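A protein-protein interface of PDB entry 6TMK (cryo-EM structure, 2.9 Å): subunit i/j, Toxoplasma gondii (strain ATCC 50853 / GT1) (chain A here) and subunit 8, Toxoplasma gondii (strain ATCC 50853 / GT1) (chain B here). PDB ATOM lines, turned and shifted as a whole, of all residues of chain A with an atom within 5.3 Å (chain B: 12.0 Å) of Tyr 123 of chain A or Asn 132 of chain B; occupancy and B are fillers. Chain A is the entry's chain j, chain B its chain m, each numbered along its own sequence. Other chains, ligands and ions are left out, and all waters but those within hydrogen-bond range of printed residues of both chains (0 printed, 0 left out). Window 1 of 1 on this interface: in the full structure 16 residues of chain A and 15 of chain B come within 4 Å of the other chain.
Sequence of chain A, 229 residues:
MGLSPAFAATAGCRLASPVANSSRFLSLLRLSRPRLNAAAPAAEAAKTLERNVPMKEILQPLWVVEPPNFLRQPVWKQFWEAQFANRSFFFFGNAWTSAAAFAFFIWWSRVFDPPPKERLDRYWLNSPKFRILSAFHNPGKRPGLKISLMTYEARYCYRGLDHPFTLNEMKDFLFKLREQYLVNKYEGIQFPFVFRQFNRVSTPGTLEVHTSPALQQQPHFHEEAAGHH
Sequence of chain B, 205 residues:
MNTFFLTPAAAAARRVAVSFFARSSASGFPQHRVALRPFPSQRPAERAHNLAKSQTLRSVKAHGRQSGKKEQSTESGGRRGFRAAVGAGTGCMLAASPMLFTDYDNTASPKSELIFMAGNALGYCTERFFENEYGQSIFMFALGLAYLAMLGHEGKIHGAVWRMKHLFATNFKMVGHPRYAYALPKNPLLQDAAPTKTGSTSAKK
Pro 115 of chain A touches just one residue of chain B: Glu 131 (3.5 Å). Of the printed residues of chain B, Arg 119 of chain A touches Glu 127 (3.6 Å) and Glu 131 (2.9 Å). Leu 120 of chain A touches none of the printed residues of chain B. Asp 121 of chain A touches none of the printed residues of chain B. Printed residues of chain B within 4 Å of Arg 122 of chain A: Glu 127 (2.3 Å). Of chain B, only Glu 127 (3.9 Å), Arg 128 (3.2 Å) and Asn 132 (3.3 Å) come within 4 Å of Tyr 123 of chain A. Trp 124 of chain A touches one residue of chain B. Of the printed residues of chain B, Ser 127 of chain A touches Glu 133. Of the printed residues of chain A, Glu 127 of chain B touches Arg 119, Arg 122 and Tyr 123. Of the printed residues of chain A, Arg 128 of chain B touches Tyr 123. Phe 130 of chain B touches none of the printed residues of chain A. Asn 132 of chain B touches just one residue of chain A: Tyr 123 (3.3 Å). Of the printed residues of chain A, Glu 133 of chain B touches Trp 124 and Ser 127. The nearest printed residue of chain A that does not touch Glu 131 of chain B is Tyr 123 of chain A (5.8 Å).
Among the printed residues, pairs that only touch across the chains: Tyr 123 of chain A with Arg 128 of chain B (3.2 Å), Tyr 123 of chain A with Asn 132 of chain B (3.3 Å), Pro 115 of chain A with Glu 131 of chain B (3.5 Å), Arg 119 of chain A with Glu 127 of chain B (3.6 Å), Trp 124 of chain A with Glu 133 of chain B (3.7 Å) and Tyr 123 of chain A with Glu 127 of chain B (3.9 Å).
The backbone carbonyl oxygen of Thr 126 of chain B is in hydrogen-bond range of the backbone NH of Glu 131 of chain B, 3.2 Å away. The backbone carbonyl oxygen of Glu 133 of chain B lies within hydrogen-bond range of the side-chain hydroxyl of Ser 137 of chain B (3.3 Å). The side-chain hydroxyl (OH) of Tyr 124 of chain B lies within hydrogen-bond range of the guanidinium group (NH1) of Arg 128 of chain B (3.3 Å).
The side-chain carboxylate (OE1) of Glu 131 of chain B lies within salt-bridge range of the guanidinium group (NH1) of Arg 119 of chain A. The side-chain carboxylate (OE1) of Glu 127 of chain B is in salt-bridge range of the guanidinium group (NH1) of Arg 122 of chain A (3.6 Å). The side-chain hydroxyl (OG) of Ser 127 of chain A sits close to the side-chain carboxylate (OE1) of Glu 133 of chain B (3.1 Å).
Of the 10 printed residues of chain A, 6 touch a printed residue of chain B. Printed residues of chain B that touch a printed residue of chain A: Glu 127, Arg 128, Glu 131, Asn 132 and Glu 133. Along chain B the printed residues that touch a printed residue of chain A span positions 127 to 133. Among the printed residues, Asp or Glu carboxylates within 4 Å of a Lys or Arg side-chain nitrogen of the other chain: Arg 119 of chain A with Glu 131 of chain B (2.9 Å) and Arg 122 of chain A with Glu 127 of chain B (2.3 Å).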
ATOM      1  N   PRO A 115      -8.151  35.926  12.274  1.00  0.00           N
ATOM      2  CA  PRO A 115      -6.931  35.941  13.052  1.00  0.00           C
ATOM      3  C   PRO A 115      -6.559  37.357  13.441  1.00  0.00           C
ATOM      4  O   PRO A 115      -7.050  38.328  12.848  1.00  0.00           O
ATOM      5  CB  PRO A 115      -5.905  35.336  12.091  1.00  0.00           C
ATOM      6  CG  PRO A 115      -6.377  35.750  10.781  1.00  0.00           C
ATOM      7  CD  PRO A 115      -7.870  35.726  10.844  1.00  0.00           C
ATOM      8  N   ARG A 119      -0.925  37.545  13.581  1.00  0.00           N
ATOM      9  CA  ARG A 119      -0.983  36.233  12.960  1.00  0.00           C
ATOM     10  C   ARG A 119      -1.555  36.300  11.550  1.00  0.00           C
ATOM     11  O   ARG A 119      -2.042  35.292  11.033  1.00  0.00           O
ATOM     12  CB  ARG A 119      -1.810  35.284  13.818  1.00  0.00           C
ATOM     13  CG  ARG A 119      -1.347  33.862  13.773  1.00  0.00           C
ATOM     14  CD  ARG A 119      -2.404  32.941  14.318  1.00  0.00           C
ATOM     15  NE  ARG A 119      -2.780  33.300  15.681  1.00  0.00           N
ATOM     16  CZ  ARG A 119      -3.977  33.081  16.205  1.00  0.00           C
ATOM     17  NH1 ARG A 119      -4.927  32.500  15.499  1.00  0.00           N
ATOM     18  NH2 ARG A 119      -4.226  33.446  17.445  1.00  0.00           N
ATOM     19  N   LEU A 120      -1.480  37.461  10.900  1.00  0.00           N
ATOM     20  CA  LEU A 120      -2.083  37.589   9.577  1.00  0.00           C
ATOM     21  C   LEU A 120      -1.189  37.005   8.488  1.00  0.00           C
ATOM     22  O   LEU A 120      -1.688  36.430   7.512  1.00  0.00           O
ATOM     23  CB  LEU A 120      -2.362  39.051   9.252  1.00  0.00           C
ATOM     24  CG  LEU A 120      -3.542  39.753   9.892  1.00  0.00           C
ATOM     25  CD1 LEU A 120      -3.418  41.221   9.597  1.00  0.00           C
ATOM     26  CD2 LEU A 120      -4.842  39.213   9.385  1.00  0.00           C
ATOM     27  N   ASP A 121       0.123  37.142   8.631  1.00  0.00           N
ATOM     28  CA  ASP A 121       1.076  36.631   7.657  1.00  0.00           C
ATOM     29  C   ASP A 121       1.338  35.144   7.807  1.00  0.00           C
ATOM     30  O   ASP A 121       2.244  34.619   7.154  1.00  0.00           O
ATOM     31  CB  ASP A 121       2.392  37.397   7.756  1.00  0.00           C
ATOM     32  CG  ASP A 121       3.099  37.163   9.063  1.00  0.00           C
ATOM     33  OD1 ASP A 121       2.497  37.427  10.123  1.00  0.00           O
ATOM     34  OD2 ASP A 121       4.259  36.706   9.041  1.00  0.00           O
ATOM     35  N   ARG A 122       0.575  34.457   8.651  1.00  0.00           N
ATOM     36  CA  ARG A 122       0.673  33.010   8.746  1.00  0.00           C
ATOM     37  C   ARG A 122      -0.090  32.340   7.611  1.00  0.00           C
ATOM     38  O   ARG A 122       0.419  31.414   6.973  1.00  0.00           O
ATOM     39  CB  ARG A 122       0.147  32.539  10.100  1.00  0.00           C
ATOM     40  CG  ARG A 122       0.634  31.179  10.515  1.00  0.00           C
ATOM     41  CD  ARG A 122       2.027  31.230  11.088  1.00  0.00           C
ATOM     42  NE  ARG A 122       2.604  29.902  11.249  1.00  0.00           N
ATOM     43  CZ  ARG A 122       2.397  29.110  12.290  1.00  0.00           C
ATOM     44  NH1 ARG A 122       1.623  29.494  13.289  1.00  0.00           N
ATOM     45  NH2 ARG A 122       2.974  27.927  12.330  1.00  0.00           N
ATOM     46  N   TYR A 123      -1.308  32.782   7.358  1.00  0.00           N
ATOM     47  CA  TYR A 123      -2.112  32.265   6.259  1.00  0.00           C
ATOM     48  C   TYR A 123      -2.737  33.344   5.390  1.00  0.00           C
ATOM     49  O   TYR A 123      -2.766  33.191   4.171  1.00  0.00           O
ATOM     50  CB  TYR A 123      -3.205  31.357   6.822  1.00  0.00           C
ATOM     51  CG  TYR A 123      -3.920  30.523   5.798  1.00  0.00           C
ATOM     52  CD1 TYR A 123      -3.570  29.206   5.602  1.00  0.00           C
ATOM     53  CD2 TYR A 123      -4.956  31.041   5.044  1.00  0.00           C
ATOM     54  CE1 TYR A 123      -4.215  28.435   4.684  1.00  0.00           C
ATOM     55  CE2 TYR A 123      -5.603  30.277   4.120  1.00  0.00           C
ATOM     56  CZ  TYR A 123      -5.233  28.975   3.940  1.00  0.00           C
ATOM     57  OH  TYR A 123      -5.891  28.211   3.012  1.00  0.00           O
ATOM     58  N   TRP A 124      -3.212  34.441   5.979  1.00  0.00           N
ATOM     59  CA  TRP A 124      -4.190  35.276   5.289  1.00  0.00           C
ATOM     60  C   TRP A 124      -3.552  36.066   4.157  1.00  0.00           C
ATOM     61  O   TRP A 124      -4.156  36.225   3.091  1.00  0.00           O
ATOM     62  CB  TRP A 124      -4.867  36.227   6.272  1.00  0.00           C
ATOM     63  CG  TRP A 124      -5.784  37.207   5.622  1.00  0.00           C
ATOM     64  CD1 TRP A 124      -5.659  38.557   5.629  1.00  0.00           C
ATOM     65  CD2 TRP A 124      -6.964  36.921   4.868  1.00  0.00           C
ATOM     66  NE1 TRP A 124      -6.675  39.131   4.927  1.00  0.00           N
ATOM     67  CE2 TRP A 124      -7.494  38.148   4.451  1.00  0.00           C
ATOM     68  CE3 TRP A 124      -7.623  35.750   4.503  1.00  0.00           C
ATOM     69  CZ2 TRP A 124      -8.641  38.239   3.692  1.00  0.00           C
ATOM     70  CZ3 TRP A 124      -8.761  35.845   3.753  1.00  0.00           C
ATOM     71  CH2 TRP A 124      -9.259  37.075   3.354  1.00  0.00           C
ATOM     72  N   LEU A 125      -2.339  36.569   4.360  1.00  0.00           N
ATOM     73  CA  LEU A 125      -1.708  37.389   3.343  1.00  0.00           C
ATOM     74  C   LEU A 125      -1.189  36.581   2.163  1.00  0.00           C
ATOM     75  O   LEU A 125      -0.729  37.174   1.184  1.00  0.00           O
ATOM     76  CB  LEU A 125      -0.573  38.190   3.972  1.00  0.00           C
ATOM     77  CG  LEU A 125      -0.987  39.043   5.167  1.00  0.00           C
ATOM     78  CD1 LEU A 125       0.196  39.745   5.757  1.00  0.00           C
ATOM     79  CD2 LEU A 125      -2.026  40.051   4.762  1.00  0.00           C
ATOM     80  N   ASN A 126      -1.263  35.256   2.227  1.00  0.00           N
ATOM     81  CA  ASN A 126      -0.896  34.382   1.123  1.00  0.00           C
ATOM     82  C   ASN A 126      -2.100  33.566   0.672  1.00  0.00           C
ATOM     83  O   ASN A 126      -1.965  32.423   0.242  1.00  0.00           O
ATOM     84  CB  ASN A 126       0.264  33.467   1.505  1.00  0.00           C
ATOM     85  CG  ASN A 126       1.422  34.216   2.087  1.00  0.00           C
ATOM     86  OD1 ASN A 126       1.681  34.154   3.287  1.00  0.00           O
ATOM     87  ND2 ASN A 126       2.142  34.921   1.239  1.00  0.00           N
ATOM     88  N   SER A 127      -3.259  34.155   0.740  1.00  0.00           N
ATOM     89  CA  SER A 127      -4.521  33.478   0.527  1.00  0.00           C
ATOM     90  C   SER A 127      -5.129  33.883  -0.806  1.00  0.00           C
ATOM     91  O   SER A 127      -5.012  35.043  -1.215  1.00  0.00           O
ATOM     92  CB  SER A 127      -5.504  33.794   1.655  1.00  0.00           C
ATOM     93  OG  SER A 127      -6.752  33.182   1.450  1.00  0.00           O
ATOM     94  N   LEU B 122      -5.521  20.978  17.449  1.00  0.00           N
ATOM     95  CA  LEU B 122      -6.615  21.908  17.189  1.00  0.00           C
ATOM     96  C   LEU B 122      -6.090  23.293  16.846  1.00  0.00           C
ATOM     97  O   LEU B 122      -6.673  23.991  16.015  1.00  0.00           O
ATOM     98  CB  LEU B 122      -7.550  21.978  18.390  1.00  0.00           C
ATOM     99  CG  LEU B 122      -8.717  20.996  18.479  1.00  0.00           C
ATOM    100  CD1 LEU B 122      -9.673  21.139  17.315  1.00  0.00           C
ATOM    101  CD2 LEU B 122      -8.209  19.587  18.559  1.00  0.00           C
ATOM    102  N   GLY B 123      -4.986  23.704  17.467  1.00  0.00           N
ATOM    103  CA  GLY B 123      -4.397  24.989  17.137  1.00  0.00           C
ATOM    104  C   GLY B 123      -3.832  25.015  15.730  1.00  0.00           C
ATOM    105  O   GLY B 123      -3.961  26.013  15.015  1.00  0.00           O
ATOM    106  N   TYR B 124      -3.202  23.919  15.317  1.00  0.00           N
ATOM    107  CA  TYR B 124      -2.709  23.805  13.953  1.00  0.00           C
ATOM    108  C   TYR B 124      -3.859  23.880  12.962  1.00  0.00           C
ATOM    109  O   TYR B 124      -3.802  24.632  11.981  1.00  0.00           O
ATOM    110  CB  TYR B 124      -1.937  22.498  13.789  1.00  0.00           C
ATOM    111  CG  TYR B 124      -1.501  22.236  12.374  1.00  0.00           C
ATOM    112  CD1 TYR B 124      -0.407  22.887  11.846  1.00  0.00           C
ATOM    113  CD2 TYR B 124      -2.189  21.354  11.561  1.00  0.00           C
ATOM    114  CE1 TYR B 124      -0.004  22.666  10.562  1.00  0.00           C
ATOM    115  CE2 TYR B 124      -1.792  21.129  10.271  1.00  0.00           C
ATOM    116  CZ  TYR B 124      -0.697  21.791   9.774  1.00  0.00           C
ATOM    117  OH  TYR B 124      -0.287  21.575   8.482  1.00  0.00           O
ATOM    118  N   CYS B 125      -4.916  23.102  13.197  1.00  0.00           N
ATOM    119  CA  CYS B 125      -6.046  23.120  12.278  1.00  0.00           C
ATOM    120  C   CYS B 125      -6.782  24.451  12.320  1.00  0.00           C
ATOM    121  O   CYS B 125      -7.415  24.831  11.332  1.00  0.00           O
ATOM    122  CB  CYS B 125      -7.005  21.970  12.581  1.00  0.00           C
ATOM    123  SG  CYS B 125      -6.267  20.330  12.608  1.00  0.00           S
ATOM    124  N   THR B 126      -6.710  25.178  13.431  1.00  0.00           N
ATOM    125  CA  THR B 126      -7.312  26.503  13.474  1.00  0.00           C
ATOM    126  C   THR B 126      -6.509  27.484  12.634  1.00  0.00           C
ATOM    127  O   THR B 126      -7.065  28.196  11.791  1.00  0.00           O
ATOM    128  CB  THR B 126      -7.412  26.998  14.917  1.00  0.00           C
ATOM    129  OG1 THR B 126      -8.250  26.122  15.673  1.00  0.00           O
ATOM    130  CG2 THR B 126      -7.983  28.394  14.959  1.00  0.00           C
ATOM    131  N   GLU B 127      -5.193  27.536  12.850  1.00  0.00           N
ATOM    132  CA  GLU B 127      -4.367  28.468  12.099  1.00  0.00           C
ATOM    133  C   GLU B 127      -4.342  28.131  10.613  1.00  0.00           C
ATOM    134  O   GLU B 127      -4.145  29.023   9.784  1.00  0.00           O
ATOM    135  CB  GLU B 127      -2.951  28.480  12.668  1.00  0.00           C
ATOM    136  CG  GLU B 127      -2.834  29.145  14.019  1.00  0.00           C
ATOM    137  CD  GLU B 127      -1.397  29.265  14.489  1.00  0.00           C
ATOM    138  OE1 GLU B 127      -1.067  28.700  15.551  1.00  0.00           O
ATOM    139  OE2 GLU B 127      -0.595  29.926  13.796  1.00  0.00           O
ATOM    140  N   ARG B 128      -4.543  26.862  10.256  1.00  0.00           N
ATOM    141  CA  ARG B 128      -4.443  26.441   8.866  1.00  0.00           C
ATOM    142  C   ARG B 128      -5.781  26.442   8.135  1.00  0.00           C
ATOM    143  O   ARG B 128      -5.837  26.824   6.963  1.00  0.00           O
ATOM    144  CB  ARG B 128      -3.822  25.048   8.793  1.00  0.00           C
ATOM    145  CG  ARG B 128      -3.462  24.598   7.402  1.00  0.00           C
ATOM    146  CD  ARG B 128      -2.010  24.768   7.091  1.00  0.00           C
ATOM    147  NE  ARG B 128      -1.768  24.782   5.652  1.00  0.00           N
ATOM    148  CZ  ARG B 128      -1.502  23.705   4.923  1.00  0.00           C
ATOM    149  NH1 ARG B 128      -1.445  22.506   5.480  1.00  0.00           N
ATOM    150  NH2 ARG B 128      -1.293  23.829   3.623  1.00  0.00           N
ATOM    151  N   PHE B 129      -6.863  26.022   8.789  1.00  0.00           N
ATOM    152  CA  PHE B 129      -8.140  25.804   8.122  1.00  0.00           C
ATOM    153  C   PHE B 129      -9.253  26.699   8.640  1.00  0.00           C
ATOM    154  O   PHE B 129      -9.905  27.384   7.845  1.00  0.00           O
ATOM    155  CB  PHE B 129      -8.557  24.334   8.274  1.00  0.00           C
ATOM    156  CG  PHE B 129      -7.483  23.356   7.920  1.00  0.00           C
ATOM    157  CD1 PHE B 129      -6.956  23.318   6.650  1.00  0.00           C
ATOM    158  CD2 PHE B 129      -6.997  22.476   8.863  1.00  0.00           C
ATOM    159  CE1 PHE B 129      -5.972  22.421   6.327  1.00  0.00           C
ATOM    160  CE2 PHE B 129      -6.011  21.582   8.543  1.00  0.00           C
ATOM    161  CZ  PHE B 129      -5.499  21.554   7.271  1.00  0.00           C
ATOM    162  N   PHE B 130      -9.495  26.717   9.953  1.00  0.00           N
ATOM    163  CA  PHE B 130     -10.774  27.202  10.460  1.00  0.00           C
ATOM    164  C   PHE B 130     -10.909  28.715  10.426  1.00  0.00           C
ATOM    165  O   PHE B 130     -12.012  29.222  10.199  1.00  0.00           O
ATOM    166  CB  PHE B 130     -11.001  26.736  11.897  1.00  0.00           C
ATOM    167  CG  PHE B 130     -10.982  25.256  12.079  1.00  0.00           C
ATOM    168  CD1 PHE B 130     -11.314  24.408  11.049  1.00  0.00           C
ATOM    169  CD2 PHE B 130     -10.640  24.714  13.298  1.00  0.00           C
ATOM    170  CE1 PHE B 130     -11.300  23.051  11.231  1.00  0.00           C
ATOM    171  CE2 PHE B 130     -10.623  23.362  13.480  1.00  0.00           C
ATOM    172  CZ  PHE B 130     -10.952  22.528  12.445  1.00  0.00           C
ATOM    173  N   GLU B 131      -9.824  29.459  10.632  1.00  0.00           N
ATOM    174  CA  GLU B 131      -9.905  30.912  10.702  1.00  0.00           C
ATOM    175  C   GLU B 131      -9.746  31.573   9.345  1.00  0.00           C
ATOM    176  O   GLU B 131      -9.337  32.734   9.268  1.00  0.00           O
ATOM    177  CB  GLU B 131      -8.888  31.459  11.705  1.00  0.00           C
ATOM    178  CG  GLU B 131      -7.443  31.390  11.306  1.00  0.00           C
ATOM    179  CD  GLU B 131      -6.517  31.758  12.446  1.00  0.00           C
ATOM    180  OE1 GLU B 131      -7.010  31.937  13.577  1.00  0.00           O
ATOM    181  OE2 GLU B 131      -5.299  31.884  12.210  1.00  0.00           O
ATOM    182  N   ASN B 132     -10.078  30.863   8.272  1.00  0.00           N
ATOM    183  CA  ASN B 132      -9.944  31.377   6.921  1.00  0.00           C
ATOM    184  C   ASN B 132     -11.135  30.901   6.088  1.00  0.00           C
ATOM    185  O   ASN B 132     -12.143  30.410   6.611  1.00  0.00           O
ATOM    186  CB  ASN B 132      -8.588  30.956   6.344  1.00  0.00           C
ATOM    187  CG  ASN B 132      -7.429  31.327   7.258  1.00  0.00           C
ATOM    188  OD1 ASN B 132      -6.725  30.456   7.777  1.00  0.00           O
ATOM    189  ND2 ASN B 132      -7.237  32.623   7.474  1.00  0.00           N
ATOM    190  N   GLU B 133     -11.010  31.054   4.768  1.00  0.00           N
ATOM    191  CA  GLU B 133     -12.120  30.768   3.865  1.00  0.00           C
ATOM    192  C   GLU B 133     -12.524  29.297   3.897  1.00  0.00           C
ATOM    193  O   GLU B 133     -13.716  28.968   3.814  1.00  0.00           O
ATOM    194  CB  GLU B 133     -11.742  31.201   2.450  1.00  0.00           C
ATOM    195  CG  GLU B 133     -10.444  30.611   1.929  1.00  0.00           C
ATOM    196  CD  GLU B 133      -9.244  31.514   2.140  1.00  0.00           C
ATOM    197  OE1 GLU B 133      -9.223  32.258   3.141  1.00  0.00           O
ATOM    198  OE2 GLU B 133      -8.315  31.471   1.309  1.00  0.00           O
ATOM    199  N   TYR B 134     -11.551  28.395   4.011  1.00  0.00           N
ATOM    200  CA  TYR B 134     -11.891  26.985   4.131  1.00  0.00           C
ATOM    201  C   TYR B 134     -12.654  26.720   5.421  1.00  0.00           C
ATOM    202  O   TYR B 134     -13.535  25.854   5.463  1.00  0.00           O
ATOM    203  CB  TYR B 134     -10.634  26.132   4.055  1.00  0.00           C
ATOM    204  CG  TYR B 134     -10.903  24.707   3.658  1.00  0.00           C
ATOM    205  CD1 TYR B 134     -11.267  24.389   2.364  1.00  0.00           C
ATOM    206  CD2 TYR B 134     -10.796  23.682   4.576  1.00  0.00           C
ATOM    207  CE1 TYR B 134     -11.518  23.094   1.997  1.00  0.00           C
ATOM    208  CE2 TYR B 134     -11.044  22.384   4.218  1.00  0.00           C
ATOM    209  CZ  TYR B 134     -11.405  22.094   2.926  1.00  0.00           C
ATOM    210  OH  TYR B 134     -11.655  20.796   2.561  1.00  0.00           O
ATOM    211  N   GLY B 135     -12.369  27.496   6.464  1.00  0.00           N
ATOM    212  CA  GLY B 135     -13.147  27.399   7.681  1.00  0.00           C
ATOM    213  C   GLY B 135     -14.558  27.910   7.517  1.00  0.00           C
ATOM    214  O   GLY B 135     -15.489  27.384   8.130  1.00  0.00           O
ATOM    215  N   GLN B 136     -14.744  28.933   6.688  1.00  0.00           N
ATOM    216  CA  GLN B 136     -16.104  29.366   6.392  1.00  0.00           C
ATOM    217  C   GLN B 136     -16.868  28.279   5.644  1.00  0.00           C
ATOM    218  O   GLN B 136     -18.060  28.053   5.897  1.00  0.00           O
ATOM    219  CB  GLN B 136     -16.070  30.669   5.601  1.00  0.00           C
ATOM    220  CG  GLN B 136     -15.717  31.864   6.447  1.00  0.00           C
ATOM    221  CD  GLN B 136     -16.789  32.159   7.483  1.00  0.00           C
ATOM    222  OE1 GLN B 136     -17.767  32.851   7.203  1.00  0.00           O
ATOM    223  NE2 GLN B 136     -16.625  31.602   8.677  1.00  0.00           N
ATOM    224  N   SER B 137     -16.192  27.588   4.728  1.00  0.00           N
ATOM    225  CA  SER B 137     -16.805  26.449   4.052  1.00  0.00           C
ATOM    226  C   SER B 137     -17.171  25.345   5.041  1.00  0.00           C
ATOM    227  O   SER B 137     -18.236  24.728   4.931  1.00  0.00           O
ATOM    228  CB  SER B 137     -15.873  25.921   2.966  1.00  0.00           C
ATOM    229  OG  SER B 137     -15.614  26.916   2.001  1.00  0.00           O
ATOM    230  N   ILE B 138     -16.304  25.088   6.020  1.00  0.00           N
ATOM    231  CA  ILE B 138     -16.583  24.059   7.019  1.00  0.00           C
ATOM    232  C   ILE B 138     -17.773  24.459   7.886  1.00  0.00           C
ATOM    233  O   ILE B 138     -18.600  23.618   8.269  1.00  0.00           O
ATOM    234  CB  ILE B 138     -15.317  23.804   7.859  1.00  0.00           C
ATOM    235  CG1 ILE B 138     -14.255  23.121   7.010  1.00  0.00           C
ATOM    236  CG2 ILE B 138     -15.613  22.936   9.044  1.00  0.00           C
ATOM    237  CD1 ILE B 138     -12.858  23.289   7.519  1.00  0.00           C
ATOM    238  N   PHE B 139     -17.873  25.741   8.223  1.00  0.00           N
ATOM    239  CA  PHE B 139     -19.019  26.227   8.982  1.00  0.00           C
ATOM    240  C   PHE B 139     -20.314  26.046   8.195  1.00  0.00           C
ATOM    241  O   PHE B 139     -21.342  25.635   8.752  1.00  0.00           O
ATOM    242  CB  PHE B 139     -18.806  27.686   9.367  1.00  0.00           C
ATOM    243  CG  PHE B 139     -19.913  28.258  10.179  1.00  0.00           C
ATOM    244  CD1 PHE B 139     -20.258  27.699  11.393  1.00  0.00           C
ATOM    245  CD2 PHE B 139     -20.604  29.361   9.738  1.00  0.00           C
ATOM    246  CE1 PHE B 139     -21.276  28.224  12.137  1.00  0.00           C
ATOM    247  CE2 PHE B 139     -21.621  29.891  10.484  1.00  0.00           C
ATOM    248  CZ  PHE B 139     -21.957  29.320  11.685  1.00  0.00           C
ATOM    249  N   MET B 140     -20.283  26.357   6.898  1.00  0.00           N
ATOM    250  CA  MET B 140     -21.444  26.104   6.051  1.00  0.00           C
ATOM    251  C   MET B 140     -21.777  24.620   6.002  1.00  0.00           C
ATOM    252  O   MET B 140     -22.950  24.243   5.932  1.00  0.00           O
ATOM    253  CB  MET B 140     -21.207  26.631   4.642  1.00  0.00           C
ATOM    254  CG  MET B 140     -21.579  28.075   4.444  1.00  0.00           C
ATOM    255  SD  MET B 140     -21.715  28.512   2.702  1.00  0.00           S
ATOM    256  CE  MET B 140     -19.998  28.780   2.292  1.00  0.00           C
ATOM    257  N   PHE B 141     -20.762  23.761   6.030  1.00  0.00           N
ATOM    258  CA  PHE B 141     -21.007  22.324   6.038  1.00  0.00           C
ATOM    259  C   PHE B 141     -21.727  21.901   7.314  1.00  0.00           C
ATOM    260  O   PHE B 141     -22.644  21.071   7.277  1.00  0.00           O
ATOM    261  CB  PHE B 141     -19.681  21.585   5.881  1.00  0.00           C
ATOM    262  CG  PHE B 141     -19.800  20.093   5.925  1.00  0.00           C
ATOM    263  CD1 PHE B 141     -20.201  19.387   4.809  1.00  0.00           C
ATOM    264  CD2 PHE B 141     -19.490  19.394   7.073  1.00  0.00           C
ATOM    265  CE1 PHE B 141     -20.302  18.015   4.844  1.00  0.00           C
ATOM    266  CE2 PHE B 141     -19.592  18.024   7.112  1.00  0.00           C
ATOM    267  CZ  PHE B 141     -19.996  17.335   5.999  1.00  0.00           C
